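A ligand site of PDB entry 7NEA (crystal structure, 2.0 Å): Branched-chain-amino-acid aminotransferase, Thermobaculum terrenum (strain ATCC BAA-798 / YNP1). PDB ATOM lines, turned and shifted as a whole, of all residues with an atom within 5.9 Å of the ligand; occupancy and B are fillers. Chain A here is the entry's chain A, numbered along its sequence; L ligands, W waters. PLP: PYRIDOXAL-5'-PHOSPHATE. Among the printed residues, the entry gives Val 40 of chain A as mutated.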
ATOM      1  N   PHE A  38      -6.017  -0.930  -5.162  1.00  0.00           N
ATOM      2  CA  PHE A  38      -5.705  -1.676  -6.387  1.00  0.00           C
ATOM      3  C   PHE A  38      -4.284  -2.227  -6.260  1.00  0.00           C
ATOM      4  O   PHE A  38      -3.523  -1.821  -5.380  1.00  0.00           O
ATOM      5  CB  PHE A  38      -5.885  -0.745  -7.600  1.00  0.00           C
ATOM      6  CG  PHE A  38      -4.775   0.278  -7.738  1.00  0.00           C
ATOM      7  CD1 PHE A  38      -4.780   1.422  -6.972  1.00  0.00           C
ATOM      8  CD2 PHE A  38      -3.746   0.101  -8.629  1.00  0.00           C
ATOM      9  CE1 PHE A  38      -3.766   2.367  -7.068  1.00  0.00           C
ATOM     10  CE2 PHE A  38      -2.729   1.036  -8.735  1.00  0.00           C
ATOM     11  CZ  PHE A  38      -2.753   2.190  -7.964  1.00  0.00           C
ATOM     12  N   GLU A  39      -3.906  -3.096  -7.185  1.00  0.00           N
ATOM     13  CA  GLU A  39      -2.553  -3.574  -7.423  1.00  0.00           C
ATOM     14  C   GLU A  39      -2.311  -3.435  -8.912  1.00  0.00           C
ATOM     15  O   GLU A  39      -3.250  -3.513  -9.720  1.00  0.00           O
ATOM     16  CB  GLU A  39      -2.373  -5.006  -6.885  1.00  0.00           C
ATOM     17  CG  GLU A  39      -2.319  -5.077  -5.397  1.00  0.00           C
ATOM     18  CD  GLU A  39      -1.022  -4.505  -4.784  1.00  0.00           C
ATOM     19  OE1 GLU A  39      -0.008  -4.508  -5.482  1.00  0.00           O
ATOM     20  OE2 GLU A  39      -1.094  -4.026  -3.629  1.00  0.00           O
ATOM     21  N   VAL A  40      -1.050  -3.344  -9.275  1.00  0.00           N
ATOM     22  CA  VAL A  40      -0.617  -3.516 -10.685  1.00  0.00           C
ATOM     23  C   VAL A  40       0.385  -4.676 -10.652  1.00  0.00           C
ATOM     24  O   VAL A  40       1.384  -4.653  -9.840  1.00  0.00           O
ATOM     25  CB  VAL A  40       0.033  -2.243 -11.258  1.00  0.00           C
ATOM     26  CG1 VAL A  40       0.578  -2.505 -12.672  1.00  0.00           C
ATOM     27  CG2 VAL A  40      -0.965  -1.093 -11.268  1.00  0.00           C
ATOM     28  N   HIS A  60       1.778  -9.390  -4.151  1.00  0.00           N
ATOM     29  CA  HIS A  60       0.787  -8.386  -4.600  1.00  0.00           C
ATOM     30  C   HIS A  60      -0.587  -8.688  -4.018  1.00  0.00           C
ATOM     31  O   HIS A  60      -1.264  -7.758  -3.602  1.00  0.00           O
ATOM     32  CB  HIS A  60       0.722  -8.311  -6.107  1.00  0.00           C
ATOM     33  CG  HIS A  60       1.817  -7.513  -6.726  1.00  0.00           C
ATOM     34  ND1 HIS A  60       1.872  -6.135  -6.602  1.00  0.00           N
ATOM     35  CD2 HIS A  60       2.933  -7.910  -7.356  1.00  0.00           C
ATOM     36  CE1 HIS A  60       2.964  -5.721  -7.253  1.00  0.00           C
ATOM     37  NE2 HIS A  60       3.664  -6.799  -7.668  1.00  0.00           N
ATOM     38  N   ARG A  63      -0.615  -7.786  -0.357  1.00  0.00           N
ATOM     39  CA  ARG A  63      -0.658  -6.323  -0.148  1.00  0.00           C
ATOM     40  C   ARG A  63      -2.071  -5.838  -0.380  1.00  0.00           C
ATOM     41  O   ARG A  63      -2.532  -4.978   0.369  1.00  0.00           O
ATOM     42  CB  ARG A  63       0.388  -5.583  -0.985  1.00  0.00           C
ATOM     43  CG  ARG A  63       0.493  -4.096  -0.610  1.00  0.00           C
ATOM     44  CD  ARG A  63       1.655  -3.348  -1.228  1.00  0.00           C
ATOM     45  NE  ARG A  63       1.440  -3.267  -2.662  1.00  0.00           N
ATOM     46  CZ  ARG A  63       2.382  -2.951  -3.558  1.00  0.00           C
ATOM     47  NH1 ARG A  63       2.088  -2.962  -4.846  1.00  0.00           N
ATOM     48  NH2 ARG A  63       3.620  -2.673  -3.189  1.00  0.00           N
ATOM     49  N   ARG A 149       3.920  15.566   0.002  1.00  0.00           N
ATOM     50  CA  ARG A 149       3.365  14.198  -0.035  1.00  0.00           C
ATOM     51  C   ARG A 149       2.464  13.980   1.200  1.00  0.00           C
ATOM     52  O   ARG A 149       2.791  14.444   2.309  1.00  0.00           O
ATOM     53  CB  ARG A 149       4.493  13.164  -0.041  1.00  0.00           C
ATOM     54  CG  ARG A 149       4.041  11.719  -0.295  1.00  0.00           C
ATOM     55  CD  ARG A 149       3.301  11.599  -1.626  1.00  0.00           C
ATOM     56  NE  ARG A 149       2.870  10.235  -1.932  1.00  0.00           N
ATOM     57  CZ  ARG A 149       1.931   9.855  -2.831  1.00  0.00           C
ATOM     58  NH1 ARG A 149       1.142  10.719  -3.480  1.00  0.00           N
ATOM     59  NH2 ARG A 149       1.747   8.556  -3.039  1.00  0.00           N
ATOM     60  N   LYS A 160      -2.634   1.370  -0.829  1.00  0.00           N
ATOM     61  CA  LYS A 160      -2.500   1.678  -2.287  1.00  0.00           C
ATOM     62  C   LYS A 160      -3.873   2.052  -2.848  1.00  0.00           C
ATOM     63  O   LYS A 160      -4.566   1.221  -3.519  1.00  0.00           O
ATOM     64  CB  LYS A 160      -1.925   0.475  -3.066  1.00  0.00           C
ATOM     65  CG  LYS A 160      -1.429   0.825  -4.456  1.00  0.00           C
ATOM     66  CD  LYS A 160      -0.509  -0.321  -4.899  1.00  0.00           C
ATOM     67  CE  LYS A 160       0.037  -0.136  -6.293  1.00  0.00           C
ATOM     68  NZ  LYS A 160       0.828   1.106  -6.414  1.00  0.00           N
ATOM     69  N   TYR A 165      -3.726   9.100  -5.326  1.00  0.00           N
ATOM     70  CA  TYR A 165      -3.252   9.708  -6.600  1.00  0.00           C
ATOM     71  C   TYR A 165      -3.788  11.128  -6.824  1.00  0.00           C
ATOM     72  O   TYR A 165      -3.283  11.798  -7.696  1.00  0.00           O
ATOM     73  CB  TYR A 165      -3.550   8.745  -7.759  1.00  0.00           C
ATOM     74  CG  TYR A 165      -2.530   7.628  -7.793  1.00  0.00           C
ATOM     75  CD1 TYR A 165      -2.648   6.489  -7.025  1.00  0.00           C
ATOM     76  CD2 TYR A 165      -1.395   7.798  -8.547  1.00  0.00           C
ATOM     77  CE1 TYR A 165      -1.635   5.529  -7.002  1.00  0.00           C
ATOM     78  CE2 TYR A 165      -0.407   6.834  -8.590  1.00  0.00           C
ATOM     79  CZ  TYR A 165      -0.522   5.696  -7.813  1.00  0.00           C
ATOM     80  OH  TYR A 165       0.492   4.805  -7.909  1.00  0.00           O
ATOM     81  N   SER A 168      -0.771  12.767  -5.863  1.00  0.00           N
ATOM     82  CA  SER A 168       0.160  12.508  -6.975  1.00  0.00           C
ATOM     83  C   SER A 168      -0.095  13.529  -8.100  1.00  0.00           C
ATOM     84  O   SER A 168       0.905  14.059  -8.684  1.00  0.00           O
ATOM     85  CB  SER A 168       0.112  11.071  -7.470  1.00  0.00           C
ATOM     86  OG  SER A 168       0.568  10.172  -6.435  1.00  0.00           O
ATOM     87  N   GLU A 194       8.986   9.840  -2.221  1.00  0.00           N
ATOM     88  CA  GLU A 194       8.919   8.881  -3.372  1.00  0.00           C
ATOM     89  C   GLU A 194       8.569   9.705  -4.613  1.00  0.00           C
ATOM     90  O   GLU A 194       8.287  10.955  -4.443  1.00  0.00           O
ATOM     91  CB  GLU A 194       7.868   7.775  -3.129  1.00  0.00           C
ATOM     92  CG  GLU A 194       6.434   8.275  -2.820  1.00  0.00           C
ATOM     93  CD  GLU A 194       5.351   7.263  -2.353  1.00  0.00           C
ATOM     94  OE1 GLU A 194       5.529   6.072  -2.558  1.00  0.00           O
ATOM     95  OE2 GLU A 194       4.317   7.684  -1.613  1.00  0.00           O
ATOM     96  N   GLY A 195       8.496   9.048  -5.777  1.00  0.00           N
ATOM     97  CA  GLY A 195       7.830   9.631  -6.946  1.00  0.00           C
ATOM     98  C   GLY A 195       6.304   9.645  -6.814  1.00  0.00           C
ATOM     99  O   GLY A 195       5.746   9.258  -5.759  1.00  0.00           O
ATOM    100  N   THR A 196       5.644  10.114  -7.868  1.00  0.00           N
ATOM    101  CA  THR A 196       4.178  10.208  -7.947  1.00  0.00           C
ATOM    102  C   THR A 196       3.587   8.799  -8.020  1.00  0.00           C
ATOM    103  O   THR A 196       2.445   8.594  -7.532  1.00  0.00           O
ATOM    104  CB  THR A 196       3.700  11.118  -9.105  1.00  0.00           C
ATOM    105  OG1 THR A 196       4.261  10.659 -10.317  1.00  0.00           O
ATOM    106  CG2 THR A 196       4.142  12.545  -8.909  1.00  0.00           C
ATOM    107  N   GLY A 197       4.298   7.838  -8.598  1.00  0.00           N
ATOM    108  CA  GLY A 197       3.763   6.475  -8.737  1.00  0.00           C
ATOM    109  C   GLY A 197       4.821   5.404  -8.505  1.00  0.00           C
ATOM    110  O   GLY A 197       4.559   4.254  -8.900  1.00  0.00           O
ATOM    111  N   SER A 198       6.009   5.726  -7.951  1.00  0.00           N
ATOM    112  CA  SER A 198       7.034   4.671  -7.829  1.00  0.00           C
ATOM    113  C   SER A 198       8.035   5.133  -6.763  1.00  0.00           C
ATOM    114  O   SER A 198       8.047   6.383  -6.507  1.00  0.00           O
ATOM    115  CB  SER A 198       7.677   4.484  -9.158  1.00  0.00           C
ATOM    116  OG  SER A 198       8.126   5.758  -9.569  1.00  0.00           O
ATOM    117  N   CYS A 199       8.869   4.209  -6.305  1.00  0.00           N
ATOM    118  CA  CYS A 199       9.911   4.592  -5.320  1.00  0.00           C
ATOM    119  C   CYS A 199      11.150   5.099  -6.083  1.00  0.00           C
ATOM    120  O   CYS A 199      11.287   4.865  -7.260  1.00  0.00           O
ATOM    121  CB  CYS A 199      10.138   3.499  -4.268  1.00  0.00           C
ATOM    122  SG  CYS A 199       8.641   3.162  -3.285  1.00  0.00           S
ATOM    123  N   LEU A 218       4.879   4.217  -0.226  1.00  0.00           N
ATOM    124  CA  LEU A 218       4.254   2.900  -0.391  1.00  0.00           C
ATOM    125  C   LEU A 218       5.375   1.857  -0.277  1.00  0.00           C
ATOM    126  O   LEU A 218       6.477   2.121  -0.807  1.00  0.00           O
ATOM    127  CB  LEU A 218       3.523   2.851  -1.728  1.00  0.00           C
ATOM    128  CG  LEU A 218       2.658   1.583  -1.793  1.00  0.00           C
ATOM    129  CD1 LEU A 218       1.208   1.972  -1.943  1.00  0.00           C
ATOM    130  CD2 LEU A 218       3.189   0.648  -2.864  1.00  0.00           C
ATOM    131  N   GLU A 219       5.128   0.783   0.440  1.00  0.00           N
ATOM    132  CA  GLU A 219       6.056  -0.374   0.556  1.00  0.00           C
ATOM    133  C   GLU A 219       6.073  -1.222  -0.756  1.00  0.00           C
ATOM    134  O   GLU A 219       5.600  -2.373  -0.795  1.00  0.00           O
ATOM    135  CB  GLU A 219       5.688  -1.266   1.738  1.00  0.00           C
ATOM    136  CG  GLU A 219       6.827  -2.238   2.055  1.00  0.00           C
ATOM    137  CD  GLU A 219       6.793  -2.796   3.470  1.00  0.00           C
ATOM    138  OE1 GLU A 219       5.840  -2.441   4.242  1.00  0.00           O
ATOM    139  OE2 GLU A 219       7.621  -3.668   3.729  1.00  0.00           O
ATOM    140  N   SER A 220       6.760  -0.672  -1.741  1.00  0.00           N
ATOM    141  CA  SER A 220       6.865  -1.193  -3.119  1.00  0.00           C
ATOM    142  C   SER A 220       7.456  -2.614  -3.111  1.00  0.00           C
ATOM    143  O   SER A 220       8.511  -2.820  -2.503  1.00  0.00           O
ATOM    144  CB  SER A 220       7.718  -0.199  -3.929  1.00  0.00           C
ATOM    145  OG  SER A 220       8.314  -0.774  -5.055  1.00  0.00           O
ATOM    146  N   ILE A 221       6.872  -3.508  -3.896  1.00  0.00           N
ATOM    147  CA  ILE A 221       7.442  -4.832  -4.228  1.00  0.00           C
ATOM    148  C   ILE A 221       8.638  -4.696  -5.183  1.00  0.00           C
ATOM    149  O   ILE A 221       9.619  -5.419  -4.985  1.00  0.00           O
ATOM    150  CB  ILE A 221       6.312  -5.733  -4.752  1.00  0.00           C
ATOM    151  CG1 ILE A 221       5.376  -6.054  -3.571  1.00  0.00           C
ATOM    152  CG2 ILE A 221       6.865  -6.983  -5.421  1.00  0.00           C
ATOM    153  CD1 ILE A 221       4.035  -6.590  -3.999  1.00  0.00           C
ATOM    154  N   THR A 222       8.620  -3.748  -6.118  1.00  0.00           N
ATOM    155  CA  THR A 222       9.798  -3.476  -6.989  1.00  0.00           C
ATOM    156  C   THR A 222      10.960  -2.970  -6.124  1.00  0.00           C
ATOM    157  O   THR A 222      12.120  -3.435  -6.342  1.00  0.00           O
ATOM    158  CB  THR A 222       9.450  -2.577  -8.181  1.00  0.00           C
ATOM    159  OG1 THR A 222       8.188  -2.943  -8.769  1.00  0.00           O
ATOM    160  CG2 THR A 222      10.571  -2.575  -9.184  1.00  0.00           C
ATOM    161  N   ARG A 223      10.690  -2.066  -5.195  1.00  0.00           N
ATOM    162  CA  ARG A 223      11.728  -1.545  -4.245  1.00  0.00           C
ATOM    163  C   ARG A 223      12.370  -2.718  -3.538  1.00  0.00           C
ATOM    164  O   ARG A 223      13.606  -2.812  -3.552  1.00  0.00           O
ATOM    165  CB  ARG A 223      11.137  -0.514  -3.292  1.00  0.00           C
ATOM    166  CG  ARG A 223      12.004  -0.046  -2.115  1.00  0.00           C
ATOM    167  CD  ARG A 223      11.034   0.805  -1.274  1.00  0.00           C
ATOM    168  NE  ARG A 223      11.758   1.469  -0.221  1.00  0.00           N
ATOM    169  CZ  ARG A 223      12.274   0.835   0.821  1.00  0.00           C
ATOM    170  NH1 ARG A 223      12.004  -0.443   1.013  1.00  0.00           N
ATOM    171  NH2 ARG A 223      12.954   1.482   1.742  1.00  0.00           N
ATOM    172  N   CYS A 257      11.495   3.166  -9.521  1.00  0.00           N
ATOM    173  CA  CYS A 257      11.163   1.724  -9.713  1.00  0.00           C
ATOM    174  C   CYS A 257       9.783   1.404  -9.147  1.00  0.00           C
ATOM    175  O   CYS A 257       9.263   2.070  -8.176  1.00  0.00           O
ATOM    176  CB  CYS A 257      12.301   0.823  -9.262  1.00  0.00           C
ATOM    177  SG  CYS A 257      12.212   0.262  -7.545  1.00  0.00           S
ATOM    178  N   GLY A 258       9.141   0.486  -9.826  1.00  0.00           N
ATOM    179  CA  GLY A 258       7.703   0.222  -9.634  1.00  0.00           C
ATOM    180  C   GLY A 258       7.262  -0.846 -10.628  1.00  0.00           C
ATOM    181  O   GLY A 258       8.020  -1.119 -11.603  1.00  0.00           O
ATOM    182  N   THR A 259       6.169  -1.541 -10.345  1.00  0.00           N
ATOM    183  CA  THR A 259       5.683  -2.556 -11.315  1.00  0.00           C
ATOM    184  C   THR A 259       5.507  -1.871 -12.694  1.00  0.00           C
ATOM    185  O   THR A 259       6.020  -2.350 -13.710  1.00  0.00           O
ATOM    186  CB  THR A 259       4.460  -3.324 -10.781  1.00  0.00           C
ATOM    187  OG1 THR A 259       4.803  -3.874  -9.485  1.00  0.00           O
ATOM    188  CG2 THR A 259       4.056  -4.402 -11.772  1.00  0.00           C
ATOM    189  N   HIS A 260       4.807  -0.752 -12.762  1.00  0.00           N
ATOM    190  CA  HIS A 260       4.575  -0.026 -14.039  1.00  0.00           C
ATOM    191  C   HIS A 260       5.891   0.637 -14.557  1.00  0.00           C
ATOM    192  O   HIS A 260       6.219   0.553 -15.732  1.00  0.00           O
ATOM    193  CB  HIS A 260       3.464   0.999 -13.761  1.00  0.00           C
ATOM    194  CG  HIS A 260       3.308   1.972 -14.874  1.00  0.00           C
ATOM    195  ND1 HIS A 260       4.017   3.196 -14.905  1.00  0.00           N
ATOM    196  CD2 HIS A 260       2.593   1.904 -16.021  1.00  0.00           C
ATOM    197  CE1 HIS A 260       3.719   3.839 -16.020  1.00  0.00           C
ATOM    198  NE2 HIS A 260       2.847   3.059 -16.724  1.00  0.00           N
HETATM  199  N1  PLP L   1       4.654   4.420  -5.134  1.00  0.00           N
HETATM  200  C2  PLP L   1       3.299   4.548  -5.146  1.00  0.00           C
HETATM  201  C2A PLP L   1       2.683   5.845  -4.722  1.00  0.00           C
HETATM  202  C3  PLP L   1       2.490   3.517  -5.640  1.00  0.00           C
HETATM  203  O3  PLP L   1       1.111   3.653  -5.721  1.00  0.00           O
HETATM  204  C4  PLP L   1       3.107   2.310  -6.082  1.00  0.00           C
HETATM  205  C4A PLP L   1       2.230   1.198  -6.510  1.00  0.00           C
HETATM  206  C5  PLP L   1       4.531   2.198  -6.040  1.00  0.00           C
HETATM  207  C6  PLP L   1       5.244   3.268  -5.536  1.00  0.00           C
HETATM  208  C5A PLP L   1       5.261   0.954  -6.507  1.00  0.00           C
HETATM  209  O4P PLP L   1       4.880  -0.312  -5.863  1.00  0.00           O
HETATM  210  P   PLP L   1       5.301  -1.818  -6.562  1.00  0.00           P
HETATM  211  O1P PLP L   1       4.490  -1.712  -7.916  1.00  0.00           O
HETATM  212  O2P PLP L   1       6.825  -1.740  -6.806  1.00  0.00           O
HETATM  213  O3P PLP L   1       4.737  -2.795  -5.552  1.00  0.00           O
HETATM  214  O   HOH W   1       3.371   0.092 -10.172  1.00  0.00           O
HETATM  215  O   HOH W   2       1.856  -2.714  -7.849  1.00  0.00           O
HETATM  216  O   HOH W   3      -0.602   4.836  -3.793  1.00  0.00           O
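NZ of Lys 160 is covalently linked to C4A of the ligand. An oxygen (O2P) of the ligand sits at hydrogen-bond distance from the side-chain hydroxyl of Ser 220 (2.5 Å). The side-chain hydroxyl of Tyr 165 lies within hydrogen-bond range of an oxygen (O3) of the ligand (2.5 Å). NH2 of Arg 63 is in salt-bridge range of O3P of the ligand, 2.6 Å away. An oxygen (O2P) of the ligand sits at hydrogen-bond distance from the backbone NH of Thr 222 (2.8 Å). The side-chain hydroxyl (OG1) of Thr 222 is in hydrogen-bond range of an oxygen (O2P) of the ligand, 2.7 Å away. O1P of the ligand sits at hydrogen-bond distance from N of Thr 259 (3.0 Å). An oxygen (O1P) of the ligand sits at hydrogen-bond distance from the side-chain hydroxyl (OG1) of Thr 259, at 2.7 Å. An oxygen (O3P) of the ligand sits at hydrogen-bond distance from the backbone NH (N) of Ile 221 (2.8 Å). The backbone NH of Ser 198 is in hydrogen-bond range of a nitrogen (N1) of the ligand (3.4 Å).
Water W2 lies within hydrogen-bond range of O of Val 40 (2.8 Å), O1P of the ligand (2.8 Å) and NH1 of Arg 63 (3.0 Å). Water W1 lies within hydrogen-bond range of N of His 260 (3.1 Å), O1P of the ligand (3.1 Å) and N of Thr 259 (3.2 Å).
The side-chain carboxylate (OE1) of Glu 194 lies close to a nitrogen (N1) of the ligand (3.2 Å). Merely in contact with the ligand: His 60, Arg 149, Thr 196, Gly 197, Cys 199, Leu 218 and Gly 258. Hydrophobic or aromatic side chains that line the ligand: His 60, Tyr 165, Leu 218 and Ile 221. Of the 25 residues printed, 16 come within 4 Å of the ligand.
N of Phe 38 sits at hydrogen-bond distance from O of Lys 160, at 3.1 Å. The side-chain hydroxyl (OG) of Ser 220 lies within hydrogen-bond range of the backbone NH (N) of Arg 223, 2.7 Å away. The backbone carbonyl oxygen (O) of Glu 219 sits at hydrogen-bond distance from the guanidinium group (NH2) of Arg 63, 3.1 Å away. The guanidinium group of Arg 63 lies within salt-bridge range of the side-chain carboxylate of Glu 39 (2.7 Å). OG1 of Thr 222 sits close to O of Gly 258 (3.4 Å). OE2 of Glu 194 is in salt-bridge range of NE of Arg 149 (3.0 Å). A ring nitrogen (ND1) of His 60 sits at hydrogen-bond distance from the side-chain carboxylate of Glu 39. O of Cys 199 lies within hydrogen-bond range of N of Cys 257 (2.8 Å).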
